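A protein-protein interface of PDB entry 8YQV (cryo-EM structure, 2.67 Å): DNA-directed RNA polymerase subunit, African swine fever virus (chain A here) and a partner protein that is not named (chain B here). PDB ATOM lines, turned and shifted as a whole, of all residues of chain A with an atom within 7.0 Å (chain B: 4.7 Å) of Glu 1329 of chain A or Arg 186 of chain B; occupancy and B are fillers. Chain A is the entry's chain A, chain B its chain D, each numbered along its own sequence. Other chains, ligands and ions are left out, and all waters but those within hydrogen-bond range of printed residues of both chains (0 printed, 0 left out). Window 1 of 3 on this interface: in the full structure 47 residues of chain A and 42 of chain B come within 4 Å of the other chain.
Of chain B, only Pro 137 (3.6 Å), His 139 (3.8 Å), Ile 184 (3.6 Å), Arg 186 (3.0 Å) and Arg 198 (2.9 Å) come within 4 Å of Glu 1329 of chain A.
Of chain A, only Glu 857, Glu 1329, Arg 1332 and Asp 1358 come within 4 Å of Arg 186 of chain B.
Printed residues of chain B within 4 Å of Gln 1333 of chain A: Pro 187 (3.1 Å).
Of the printed residues of chain A, His 139 of chain B touches Glu 1329 (3.8 Å).
Of the printed residues of chain B, Ile 911 of chain A touches Pro 187 and His 193.
The nearest residue of chain B that does not touch Glu 1329 of chain A is Val 196 of chain B (4.4 Å).
The guanidinium group of Arg 198 of chain B lies within salt-bridge range of the side-chain carboxylate of Glu 1329 of chain A (2.9 Å).
OE2 of Glu 857 of chain A is in salt-bridge range of NE of Arg 186 of chain B (3.9 Å).
NE2 of Gln 1333 of chain A sits at hydrogen-bond distance from O of Pro 187 of chain B (3.1 Å).
OG of Ser 188 of chain B sits close to OE1 of Glu 857 of chain A, 2.3 Å away.
The guanidinium group of Arg 186 of chain B is in salt-bridge range of the side-chain carboxylate of Asp 1358 of chain A.
NH2 of Arg 198 of chain B sits at hydrogen-bond distance from O of Thr 1361 of chain A (3.1 Å).
The guanidinium group (NE) of Arg 1332 of chain A lies close to the guanidinium group (NH1) of Arg 186 of chain B, at 3.4 Å.
The side-chain carboxylate (OE1) of Glu 1329 of chain A lies within salt-bridge range of the guanidinium group (NH1) of Arg 186 of chain B (3.0 Å).
NH2 of Arg 1332 of chain A lies within salt-bridge range of OE2 of Glu 857 of chain A (3.1 Å).
The backbone NH of Ile 184 of chain B sits at hydrogen-bond distance from the backbone carbonyl oxygen of Val 196 of chain B (2.9 Å).
A ring nitrogen (ND1) of His 139 of chain B lies within hydrogen-bond range of the backbone carbonyl oxygen (O) of Pro 137 of chain B (3.0 Å).
The guanidinium group (NH2) of Arg 1332 of chain A lies close to the side-chain amide nitrogen (NE2) of Gln 1333 of chain A, at 3.5 Å.
N of Arg 186 of chain B is in hydrogen-bond range of O of Ala 194 of chain B.
OD1 of Asp 1358 of chain A lies within salt-bridge range of NH1 of Arg 1332 of chain A.
Printed residues of chain B that touch a printed residue of chain A: Pro 137, His 139, Ile 184, Arg 186, Pro 187, Ser 188, His 193, Ala 194 and Arg 198.
Of the 20 printed residues of chain A, 8 touch a printed residue of chain B.
Printed residues of chain A that touch a printed residue of chain B: Glu 857, Ile 911, Glu 1329, Arg 1332, Gln 1333, Asp 1358, Thr 1361 and Gly 1364.
Hydrophobic or aromatic side chains of chain A within 4 Å of the printed part of chain B: Ile 911.
Among the printed residues, Asp or Glu carboxylates within 4 Å of a Lys or Arg side-chain nitrogen of the other chain: Glu 857 of chain A with Arg 186 of chain B, Glu 1329 of chain A with Arg 186 of chain B, Glu 1329 of chain A with Arg 198 of chain B and Asp 1358 of chain A with Arg 186 of chain B.
Ala 194 of chain B touches Glu 857 of chain A.
CB of Pro 187 of chain B touches CG2 of Ile 911 of chain A, at 3.97 Å.
CB of His 193 of chain B touches CD1 of Ile 911 of chain A, at 3.99 Å.
CD of Pro 137 of chain B touches CB of Glu 1329 of chain A, at 3.6 Å.
CG of Glu 1329 of chain A touches NE2 of His 139 of chain B, 3.8 Å away.
CD1 of Ile 184 of chain B touches OE2 of Glu 1329 of chain A, at 3.6 Å.
Gly 1364 of chain A touches Arg 198 of chain B.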
ATOM      1  N   VAL A 851       0.193 -16.922   7.832  1.00  0.00           N
ATOM      2  CA  VAL A 851       0.633 -15.556   7.604  1.00  0.00           C
ATOM      3  C   VAL A 851      -0.509 -14.691   7.092  1.00  0.00           C
ATOM      4  O   VAL A 851      -0.657 -13.543   7.505  1.00  0.00           O
ATOM      5  CB  VAL A 851       1.831 -15.539   6.632  1.00  0.00           C
ATOM      6  CG1 VAL A 851       2.183 -14.134   6.241  1.00  0.00           C
ATOM      7  CG2 VAL A 851       3.015 -16.209   7.259  1.00  0.00           C
ATOM      8  N   GLN A 852      -1.334 -15.243   6.212  1.00  0.00           N
ATOM      9  CA  GLN A 852      -2.541 -14.605   5.717  1.00  0.00           C
ATOM     10  C   GLN A 852      -3.678 -15.612   5.727  1.00  0.00           C
ATOM     11  O   GLN A 852      -3.480 -16.779   5.391  1.00  0.00           O
ATOM     12  CB  GLN A 852      -2.346 -14.065   4.303  1.00  0.00           C
ATOM     13  CG  GLN A 852      -1.662 -12.728   4.238  1.00  0.00           C
ATOM     14  CD  GLN A 852      -1.439 -12.265   2.831  1.00  0.00           C
ATOM     15  OE1 GLN A 852      -1.511 -13.047   1.897  1.00  0.00           O
ATOM     16  NE2 GLN A 852      -1.192 -10.981   2.664  1.00  0.00           N
ATOM     17  N   GLN A 853      -4.868 -15.160   6.120  1.00  0.00           N
ATOM     18  CA  GLN A 853      -6.039 -16.027   6.063  1.00  0.00           C
ATOM     19  C   GLN A 853      -6.473 -16.287   4.629  1.00  0.00           C
ATOM     20  O   GLN A 853      -6.982 -17.366   4.324  1.00  0.00           O
ATOM     21  CB  GLN A 853      -7.181 -15.409   6.861  1.00  0.00           C
ATOM     22  CG  GLN A 853      -8.399 -16.280   6.972  1.00  0.00           C
ATOM     23  CD  GLN A 853      -8.157 -17.497   7.816  1.00  0.00           C
ATOM     24  OE1 GLN A 853      -7.603 -17.399   8.905  1.00  0.00           O
ATOM     25  NE2 GLN A 853      -8.567 -18.653   7.327  1.00  0.00           N
ATOM     26  N   LEU A 854      -6.301 -15.313   3.747  1.00  0.00           N
ATOM     27  CA  LEU A 854      -6.520 -15.485   2.322  1.00  0.00           C
ATOM     28  C   LEU A 854      -5.453 -14.677   1.614  1.00  0.00           C
ATOM     29  O   LEU A 854      -5.138 -13.570   2.042  1.00  0.00           O
ATOM     30  CB  LEU A 854      -7.915 -15.023   1.905  1.00  0.00           C
ATOM     31  CG  LEU A 854      -8.439 -15.447   0.535  1.00  0.00           C
ATOM     32  CD1 LEU A 854      -8.697 -16.928   0.472  1.00  0.00           C
ATOM     33  CD2 LEU A 854      -9.702 -14.704   0.250  1.00  0.00           C
ATOM     34  N   GLU A 857      -6.009 -11.060   0.618  1.00  0.00           N
ATOM     35  CA  GLU A 857      -7.340 -10.831   1.167  1.00  0.00           C
ATOM     36  C   GLU A 857      -8.432 -11.005   0.132  1.00  0.00           C
ATOM     37  O   GLU A 857      -9.605 -10.885   0.471  1.00  0.00           O
ATOM     38  CB  GLU A 857      -7.479  -9.451   1.819  1.00  0.00           C
ATOM     39  CG  GLU A 857      -6.736  -9.333   3.123  1.00  0.00           C
ATOM     40  CD  GLU A 857      -6.190  -7.954   3.354  1.00  0.00           C
ATOM     41  OE1 GLU A 857      -6.244  -7.134   2.418  1.00  0.00           O
ATOM     42  OE2 GLU A 857      -5.695  -7.689   4.464  1.00  0.00           O
ATOM     43  N   ILE A 911     -15.778   2.498   4.404  1.00  0.00           N
ATOM     44  CA  ILE A 911     -14.499   1.810   4.540  1.00  0.00           C
ATOM     45  C   ILE A 911     -13.362   2.678   4.026  1.00  0.00           C
ATOM     46  O   ILE A 911     -12.353   2.876   4.709  1.00  0.00           O
ATOM     47  CB  ILE A 911     -14.535   0.456   3.813  1.00  0.00           C
ATOM     48  CG1 ILE A 911     -15.377  -0.544   4.598  1.00  0.00           C
ATOM     49  CG2 ILE A 911     -13.137  -0.060   3.616  1.00  0.00           C
ATOM     50  CD1 ILE A 911     -15.851  -1.710   3.784  1.00  0.00           C
ATOM     51  N   THR A1322       3.077   3.745  16.421  1.00  0.00           N
ATOM     52  CA  THR A1322       1.731   3.247  16.166  1.00  0.00           C
ATOM     53  C   THR A1322       1.493   1.910  16.853  1.00  0.00           C
ATOM     54  O   THR A1322       0.409   1.667  17.392  1.00  0.00           O
ATOM     55  CB  THR A1322       1.504   3.121  14.665  1.00  0.00           C
ATOM     56  OG1 THR A1322       1.933   4.325  14.020  1.00  0.00           O
ATOM     57  CG2 THR A1322       0.043   2.893  14.368  1.00  0.00           C
ATOM     58  N   MET A1323       2.490   1.024  16.831  1.00  0.00           N
ATOM     59  CA  MET A1323       2.359  -0.265  17.500  1.00  0.00           C
ATOM     60  C   MET A1323       2.225  -0.093  19.004  1.00  0.00           C
ATOM     61  O   MET A1323       1.392  -0.744  19.643  1.00  0.00           O
ATOM     62  CB  MET A1323       3.564  -1.140  17.167  1.00  0.00           C
ATOM     63  CG  MET A1323       3.701  -2.405  17.988  1.00  0.00           C
ATOM     64  SD  MET A1323       2.403  -3.608  17.711  1.00  0.00           S
ATOM     65  CE  MET A1323       2.525  -4.585  19.192  1.00  0.00           C
ATOM     66  N   TYR A1326      -1.427   1.824  19.511  1.00  0.00           N
ATOM     67  CA  TYR A1326      -2.663   1.369  18.886  1.00  0.00           C
ATOM     68  C   TYR A1326      -2.787  -0.142  18.776  1.00  0.00           C
ATOM     69  O   TYR A1326      -3.898  -0.665  18.844  1.00  0.00           O
ATOM     70  CB  TYR A1326      -2.793   1.989  17.491  1.00  0.00           C
ATOM     71  CG  TYR A1326      -3.021   3.485  17.482  1.00  0.00           C
ATOM     72  CD1 TYR A1326      -3.735   4.107  18.494  1.00  0.00           C
ATOM     73  CD2 TYR A1326      -2.510   4.272  16.468  1.00  0.00           C
ATOM     74  CE1 TYR A1326      -3.942   5.465  18.485  1.00  0.00           C
ATOM     75  CE2 TYR A1326      -2.708   5.629  16.452  1.00  0.00           C
ATOM     76  CZ  TYR A1326      -3.424   6.222  17.461  1.00  0.00           C
ATOM     77  OH  TYR A1326      -3.623   7.582  17.442  1.00  0.00           O
ATOM     78  N   GLY A1327      -1.689  -0.864  18.588  1.00  0.00           N
ATOM     79  CA  GLY A1327      -1.737  -2.306  18.521  1.00  0.00           C
ATOM     80  C   GLY A1327      -1.060  -2.827  17.277  1.00  0.00           C
ATOM     81  O   GLY A1327      -0.468  -2.076  16.498  1.00  0.00           O
ATOM     82  N   ILE A1328      -1.155  -4.139  17.078  1.00  0.00           N
ATOM     83  CA  ILE A1328      -0.494  -4.776  15.945  1.00  0.00           C
ATOM     84  C   ILE A1328      -1.293  -4.626  14.656  1.00  0.00           C
ATOM     85  O   ILE A1328      -0.711  -4.613  13.569  1.00  0.00           O
ATOM     86  CB  ILE A1328      -0.207  -6.258  16.250  1.00  0.00           C
ATOM     87  CG1 ILE A1328       0.746  -6.839  15.214  1.00  0.00           C
ATOM     88  CG2 ILE A1328      -1.480  -7.066  16.302  1.00  0.00           C
ATOM     89  CD1 ILE A1328       2.102  -6.204  15.225  1.00  0.00           C
ATOM     90  N   GLU A1329      -2.613  -4.514  14.743  1.00  0.00           N
ATOM     91  CA  GLU A1329      -3.405  -4.363  13.532  1.00  0.00           C
ATOM     92  C   GLU A1329      -3.266  -2.969  12.941  1.00  0.00           C
ATOM     93  O   GLU A1329      -3.303  -2.807  11.719  1.00  0.00           O
ATOM     94  CB  GLU A1329      -4.861  -4.693  13.825  1.00  0.00           C
ATOM     95  CG  GLU A1329      -5.095  -6.166  14.035  1.00  0.00           C
ATOM     96  CD  GLU A1329      -4.952  -6.955  12.755  1.00  0.00           C
ATOM     97  OE1 GLU A1329      -5.305  -6.425  11.684  1.00  0.00           O
ATOM     98  OE2 GLU A1329      -4.480  -8.105  12.815  1.00  0.00           O
ATOM     99  N   ALA A1330      -3.108  -1.954  13.790  1.00  0.00           N
ATOM    100  CA  ALA A1330      -2.811  -0.617  13.300  1.00  0.00           C
ATOM    101  C   ALA A1330      -1.370  -0.498  12.832  1.00  0.00           C
ATOM    102  O   ALA A1330      -1.075   0.315  11.953  1.00  0.00           O
ATOM    103  CB  ALA A1330      -3.101   0.409  14.386  1.00  0.00           C
ATOM    104  N   ALA A1331      -0.458  -1.275  13.415  1.00  0.00           N
ATOM    105  CA  ALA A1331       0.911  -1.312  12.914  1.00  0.00           C
ATOM    106  C   ALA A1331       1.005  -2.065  11.595  1.00  0.00           C
ATOM    107  O   ALA A1331       1.908  -1.797  10.798  1.00  0.00           O
ATOM    108  CB  ALA A1331       1.838  -1.943  13.946  1.00  0.00           C
ATOM    109  N   ARG A1332       0.104  -3.016  11.352  1.00  0.00           N
ATOM    110  CA  ARG A1332       0.080  -3.698  10.065  1.00  0.00           C
ATOM    111  C   ARG A1332      -0.319  -2.745   8.952  1.00  0.00           C
ATOM    112  O   ARG A1332       0.281  -2.748   7.875  1.00  0.00           O
ATOM    113  CB  ARG A1332      -0.877  -4.884  10.110  1.00  0.00           C
ATOM    114  CG  ARG A1332      -0.716  -5.835   8.948  1.00  0.00           C
ATOM    115  CD  ARG A1332      -1.922  -6.710   8.802  1.00  0.00           C
ATOM    116  NE  ARG A1332      -2.971  -6.046   8.043  1.00  0.00           N
ATOM    117  CZ  ARG A1332      -3.218  -6.263   6.761  1.00  0.00           C
ATOM    118  NH1 ARG A1332      -2.529  -7.148   6.065  1.00  0.00           N
ATOM    119  NH2 ARG A1332      -4.191  -5.584   6.166  1.00  0.00           N
ATOM    120  N   GLN A1333      -1.346  -1.929   9.190  1.00  0.00           N
ATOM    121  CA  GLN A1333      -1.734  -0.924   8.211  1.00  0.00           C
ATOM    122  C   GLN A1333      -0.653   0.126   8.028  1.00  0.00           C
ATOM    123  O   GLN A1333      -0.472   0.641   6.922  1.00  0.00           O
ATOM    124  CB  GLN A1333      -3.037  -0.255   8.628  1.00  0.00           C
ATOM    125  CG  GLN A1333      -4.261  -1.121   8.539  1.00  0.00           C
ATOM    126  CD  GLN A1333      -4.624  -1.478   7.116  1.00  0.00           C
ATOM    127  OE1 GLN A1333      -4.160  -0.856   6.167  1.00  0.00           O
ATOM    128  NE2 GLN A1333      -5.496  -2.462   6.963  1.00  0.00           N
ATOM    129  N   LYS A1334       0.063   0.465   9.097  1.00  0.00           N
ATOM    130  CA  LYS A1334       1.121   1.461   8.998  1.00  0.00           C
ATOM    131  C   LYS A1334       2.277   0.962   8.148  1.00  0.00           C
ATOM    132  O   LYS A1334       2.873   1.735   7.394  1.00  0.00           O
ATOM    133  CB  LYS A1334       1.600   1.852  10.394  1.00  0.00           C
ATOM    134  CG  LYS A1334       2.533   3.051  10.442  1.00  0.00           C
ATOM    135  CD  LYS A1334       1.961   4.248   9.711  1.00  0.00           C
ATOM    136  CE  LYS A1334       0.668   4.724  10.334  1.00  0.00           C
ATOM    137  NZ  LYS A1334       0.058   5.816   9.542  1.00  0.00           N
ATOM    138  N   ASP A1358       1.901  -8.605   6.574  1.00  0.00           N
ATOM    139  CA  ASP A1358       1.341  -9.753   7.271  1.00  0.00           C
ATOM    140  C   ASP A1358       2.419 -10.682   7.801  1.00  0.00           C
ATOM    141  O   ASP A1358       2.198 -11.369   8.800  1.00  0.00           O
ATOM    142  CB  ASP A1358       0.397 -10.514   6.348  1.00  0.00           C
ATOM    143  CG  ASP A1358      -1.023 -10.015   6.442  1.00  0.00           C
ATOM    144  OD1 ASP A1358      -1.792 -10.536   7.275  1.00  0.00           O
ATOM    145  OD2 ASP A1358      -1.372  -9.092   5.683  1.00  0.00           O
ATOM    146  N   THR A1361       4.179  -8.956  11.028  1.00  0.00           N
ATOM    147  CA  THR A1361       3.326  -8.775  12.196  1.00  0.00           C
ATOM    148  C   THR A1361       2.602 -10.056  12.588  1.00  0.00           C
ATOM    149  O   THR A1361       1.656 -10.004  13.374  1.00  0.00           O
ATOM    150  CB  THR A1361       2.300  -7.669  11.949  1.00  0.00           C
ATOM    151  OG1 THR A1361       1.473  -8.026  10.839  1.00  0.00           O
ATOM    152  CG2 THR A1361       2.983  -6.352  11.651  1.00  0.00           C
ATOM    153  N   GLY A1364       2.423 -11.138  16.487  1.00  0.00           N
ATOM    154  CA  GLY A1364       1.860 -10.212  17.439  1.00  0.00           C
ATOM    155  C   GLY A1364       2.725  -9.005  17.695  1.00  0.00           C
ATOM    156  O   GLY A1364       2.251  -8.034  18.292  1.00  0.00           O
ATOM    157  N   PRO B 137      -8.648  -1.442  13.624  1.00  0.00           N
ATOM    158  CA  PRO B 137      -9.777  -2.172  13.039  1.00  0.00           C
ATOM    159  C   PRO B 137     -10.757  -2.597  14.115  1.00  0.00           C
ATOM    160  O   PRO B 137     -10.564  -2.348  15.303  1.00  0.00           O
ATOM    161  CB  PRO B 137      -9.115  -3.382  12.379  1.00  0.00           C
ATOM    162  CG  PRO B 137      -7.698  -3.013  12.234  1.00  0.00           C
ATOM    163  CD  PRO B 137      -7.377  -2.139  13.388  1.00  0.00           C
ATOM    164  N   HIS B 139     -12.231  -5.042  16.544  1.00  0.00           N
ATOM    165  CA  HIS B 139     -11.893  -6.260  17.261  1.00  0.00           C
ATOM    166  C   HIS B 139     -13.121  -6.804  17.975  1.00  0.00           C
ATOM    167  O   HIS B 139     -14.005  -6.053  18.388  1.00  0.00           O
ATOM    168  CB  HIS B 139     -10.785  -5.999  18.275  1.00  0.00           C
ATOM    169  CG  HIS B 139      -9.458  -5.698  17.661  1.00  0.00           C
ATOM    170  ND1 HIS B 139      -9.238  -4.596  16.870  1.00  0.00           N
ATOM    171  CD2 HIS B 139      -8.270  -6.332  17.757  1.00  0.00           C
ATOM    172  CE1 HIS B 139      -7.977  -4.575  16.484  1.00  0.00           C
ATOM    173  NE2 HIS B 139      -7.367  -5.618  17.011  1.00  0.00           N
ATOM    174  N   ILE B 184     -11.023 -10.104  13.963  1.00  0.00           N
ATOM    175  CA  ILE B 184     -10.717  -8.736  13.584  1.00  0.00           C
ATOM    176  C   ILE B 184     -11.261  -8.492  12.188  1.00  0.00           C
ATOM    177  O   ILE B 184     -10.990  -9.265  11.264  1.00  0.00           O
ATOM    178  CB  ILE B 184      -9.205  -8.465  13.635  1.00  0.00           C
ATOM    179  CG1 ILE B 184      -8.664  -8.838  15.009  1.00  0.00           C
ATOM    180  CG2 ILE B 184      -8.917  -7.019  13.311  1.00  0.00           C
ATOM    181  CD1 ILE B 184      -7.196  -9.027  15.044  1.00  0.00           C
ATOM    182  N   GLU B 185     -12.039  -7.428  12.045  1.00  0.00           N
ATOM    183  CA  GLU B 185     -12.553  -6.972  10.765  1.00  0.00           C
ATOM    184  C   GLU B 185     -11.763  -5.740  10.356  1.00  0.00           C
ATOM    185  O   GLU B 185     -11.812  -4.715  11.049  1.00  0.00           O
ATOM    186  CB  GLU B 185     -14.042  -6.654  10.860  1.00  0.00           C
ATOM    187  CG  GLU B 185     -14.636  -6.170   9.568  1.00  0.00           C
ATOM    188  CD  GLU B 185     -15.417  -7.251   8.867  1.00  0.00           C
ATOM    189  OE1 GLU B 185     -16.127  -8.013   9.555  1.00  0.00           O
ATOM    190  OE2 GLU B 185     -15.305  -7.355   7.632  1.00  0.00           O
ATOM    191  N   ARG B 186     -11.035  -5.842   9.243  1.00  0.00           N
ATOM    192  CA  ARG B 186     -10.142  -4.762   8.881  1.00  0.00           C
ATOM    193  C   ARG B 186     -10.389  -4.280   7.459  1.00  0.00           C
ATOM    194  O   ARG B 186     -10.796  -5.058   6.593  1.00  0.00           O
ATOM    195  CB  ARG B 186      -8.670  -5.171   9.020  1.00  0.00           C
ATOM    196  CG  ARG B 186      -8.185  -6.317   8.169  1.00  0.00           C
ATOM    197  CD  ARG B 186      -7.081  -7.047   8.909  1.00  0.00           C
ATOM    198  NE  ARG B 186      -6.566  -8.206   8.193  1.00  0.00           N
ATOM    199  CZ  ARG B 186      -5.455  -8.849   8.523  1.00  0.00           C
ATOM    200  NH1 ARG B 186      -4.754  -8.517   9.592  1.00  0.00           N
ATOM    201  NH2 ARG B 186      -5.029  -9.845   7.754  1.00  0.00           N
ATOM    202  N   PRO B 187     -10.164  -2.994   7.198  1.00  0.00           N
ATOM    203  CA  PRO B 187     -10.282  -2.492   5.829  1.00  0.00           C
ATOM    204  C   PRO B 187      -9.214  -3.089   4.934  1.00  0.00           C
ATOM    205  O   PRO B 187      -8.068  -3.281   5.344  1.00  0.00           O
ATOM    206  CB  PRO B 187     -10.088  -0.981   5.989  1.00  0.00           C
ATOM    207  CG  PRO B 187     -10.294  -0.716   7.422  1.00  0.00           C
ATOM    208  CD  PRO B 187      -9.814  -1.921   8.136  1.00  0.00           C
ATOM    209  N   SER B 188      -9.595  -3.366   3.698  1.00  0.00           N
ATOM    210  CA  SER B 188      -8.681  -3.910   2.713  1.00  0.00           C
ATOM    211  C   SER B 188      -8.769  -3.060   1.461  1.00  0.00           C
ATOM    212  O   SER B 188      -9.860  -2.657   1.056  1.00  0.00           O
ATOM    213  CB  SER B 188      -9.012  -5.368   2.400  1.00  0.00           C
ATOM    214  OG  SER B 188      -8.034  -5.948   1.565  1.00  0.00           O
ATOM    215  N   HIS B 193     -12.736  -5.219   2.394  1.00  0.00           N
ATOM    216  CA  HIS B 193     -12.619  -5.512   3.819  1.00  0.00           C
ATOM    217  C   HIS B 193     -12.390  -7.002   3.987  1.00  0.00           C
ATOM    218  O   HIS B 193     -12.806  -7.801   3.149  1.00  0.00           O
ATOM    219  CB  HIS B 193     -13.837  -5.052   4.640  1.00  0.00           C
ATOM    220  CG  HIS B 193     -15.139  -5.664   4.237  1.00  0.00           C
ATOM    221  ND1 HIS B 193     -15.540  -5.783   2.928  1.00  0.00           N
ATOM    222  CD2 HIS B 193     -16.173  -6.107   4.985  1.00  0.00           C
ATOM    223  CE1 HIS B 193     -16.742  -6.326   2.885  1.00  0.00           C
ATOM    224  NE2 HIS B 193     -17.151  -6.528   4.121  1.00  0.00           N
ATOM    225  N   ALA B 194     -11.731  -7.359   5.086  1.00  0.00           N
ATOM    226  CA  ALA B 194     -11.292  -8.721   5.338  1.00  0.00           C
ATOM    227  C   ALA B 194     -11.532  -9.064   6.796  1.00  0.00           C
ATOM    228  O   ALA B 194     -11.663  -8.186   7.646  1.00  0.00           O
ATOM    229  CB  ALA B 194      -9.815  -8.901   4.998  1.00  0.00           C
ATOM    230  N   VAL B 196      -9.980 -11.655   9.877  1.00  0.00           N
ATOM    231  CA  VAL B 196      -9.007 -12.617  10.374  1.00  0.00           C
ATOM    232  C   VAL B 196      -9.384 -13.005  11.792  1.00  0.00           C
ATOM    233  O   VAL B 196     -10.225 -12.381  12.430  1.00  0.00           O
ATOM    234  CB  VAL B 196      -7.563 -12.090  10.327  1.00  0.00           C
ATOM    235  CG1 VAL B 196      -7.118 -11.948   8.905  1.00  0.00           C
ATOM    236  CG2 VAL B 196      -7.468 -10.784  11.048  1.00  0.00           C
ATOM    237  N   ARG B 198      -7.303 -14.072  15.368  1.00  0.00           N
ATOM    238  CA  ARG B 198      -6.025 -14.140  16.048  1.00  0.00           C
ATOM    239  C   ARG B 198      -6.185 -14.841  17.386  1.00  0.00           C
ATOM    240  O   ARG B 198      -7.265 -14.868  17.978  1.00  0.00           O
ATOM    241  CB  ARG B 198      -5.432 -12.748  16.255  1.00  0.00           C
ATOM    242  CG  ARG B 198      -4.767 -12.183  15.028  1.00  0.00           C
ATOM    243  CD  ARG B 198      -4.080 -10.884  15.331  1.00  0.00           C
ATOM    244  NE  ARG B 198      -3.312 -10.407  14.194  1.00  0.00           N
ATOM    245  CZ  ARG B 198      -1.998 -10.512  14.081  1.00  0.00           C
ATOM    246  NH1 ARG B 198      -1.264 -11.050  15.033  1.00  0.00           N
ATOM    247  NH2 ARG B 198      -1.404 -10.052  12.988  1.00  0.00           N
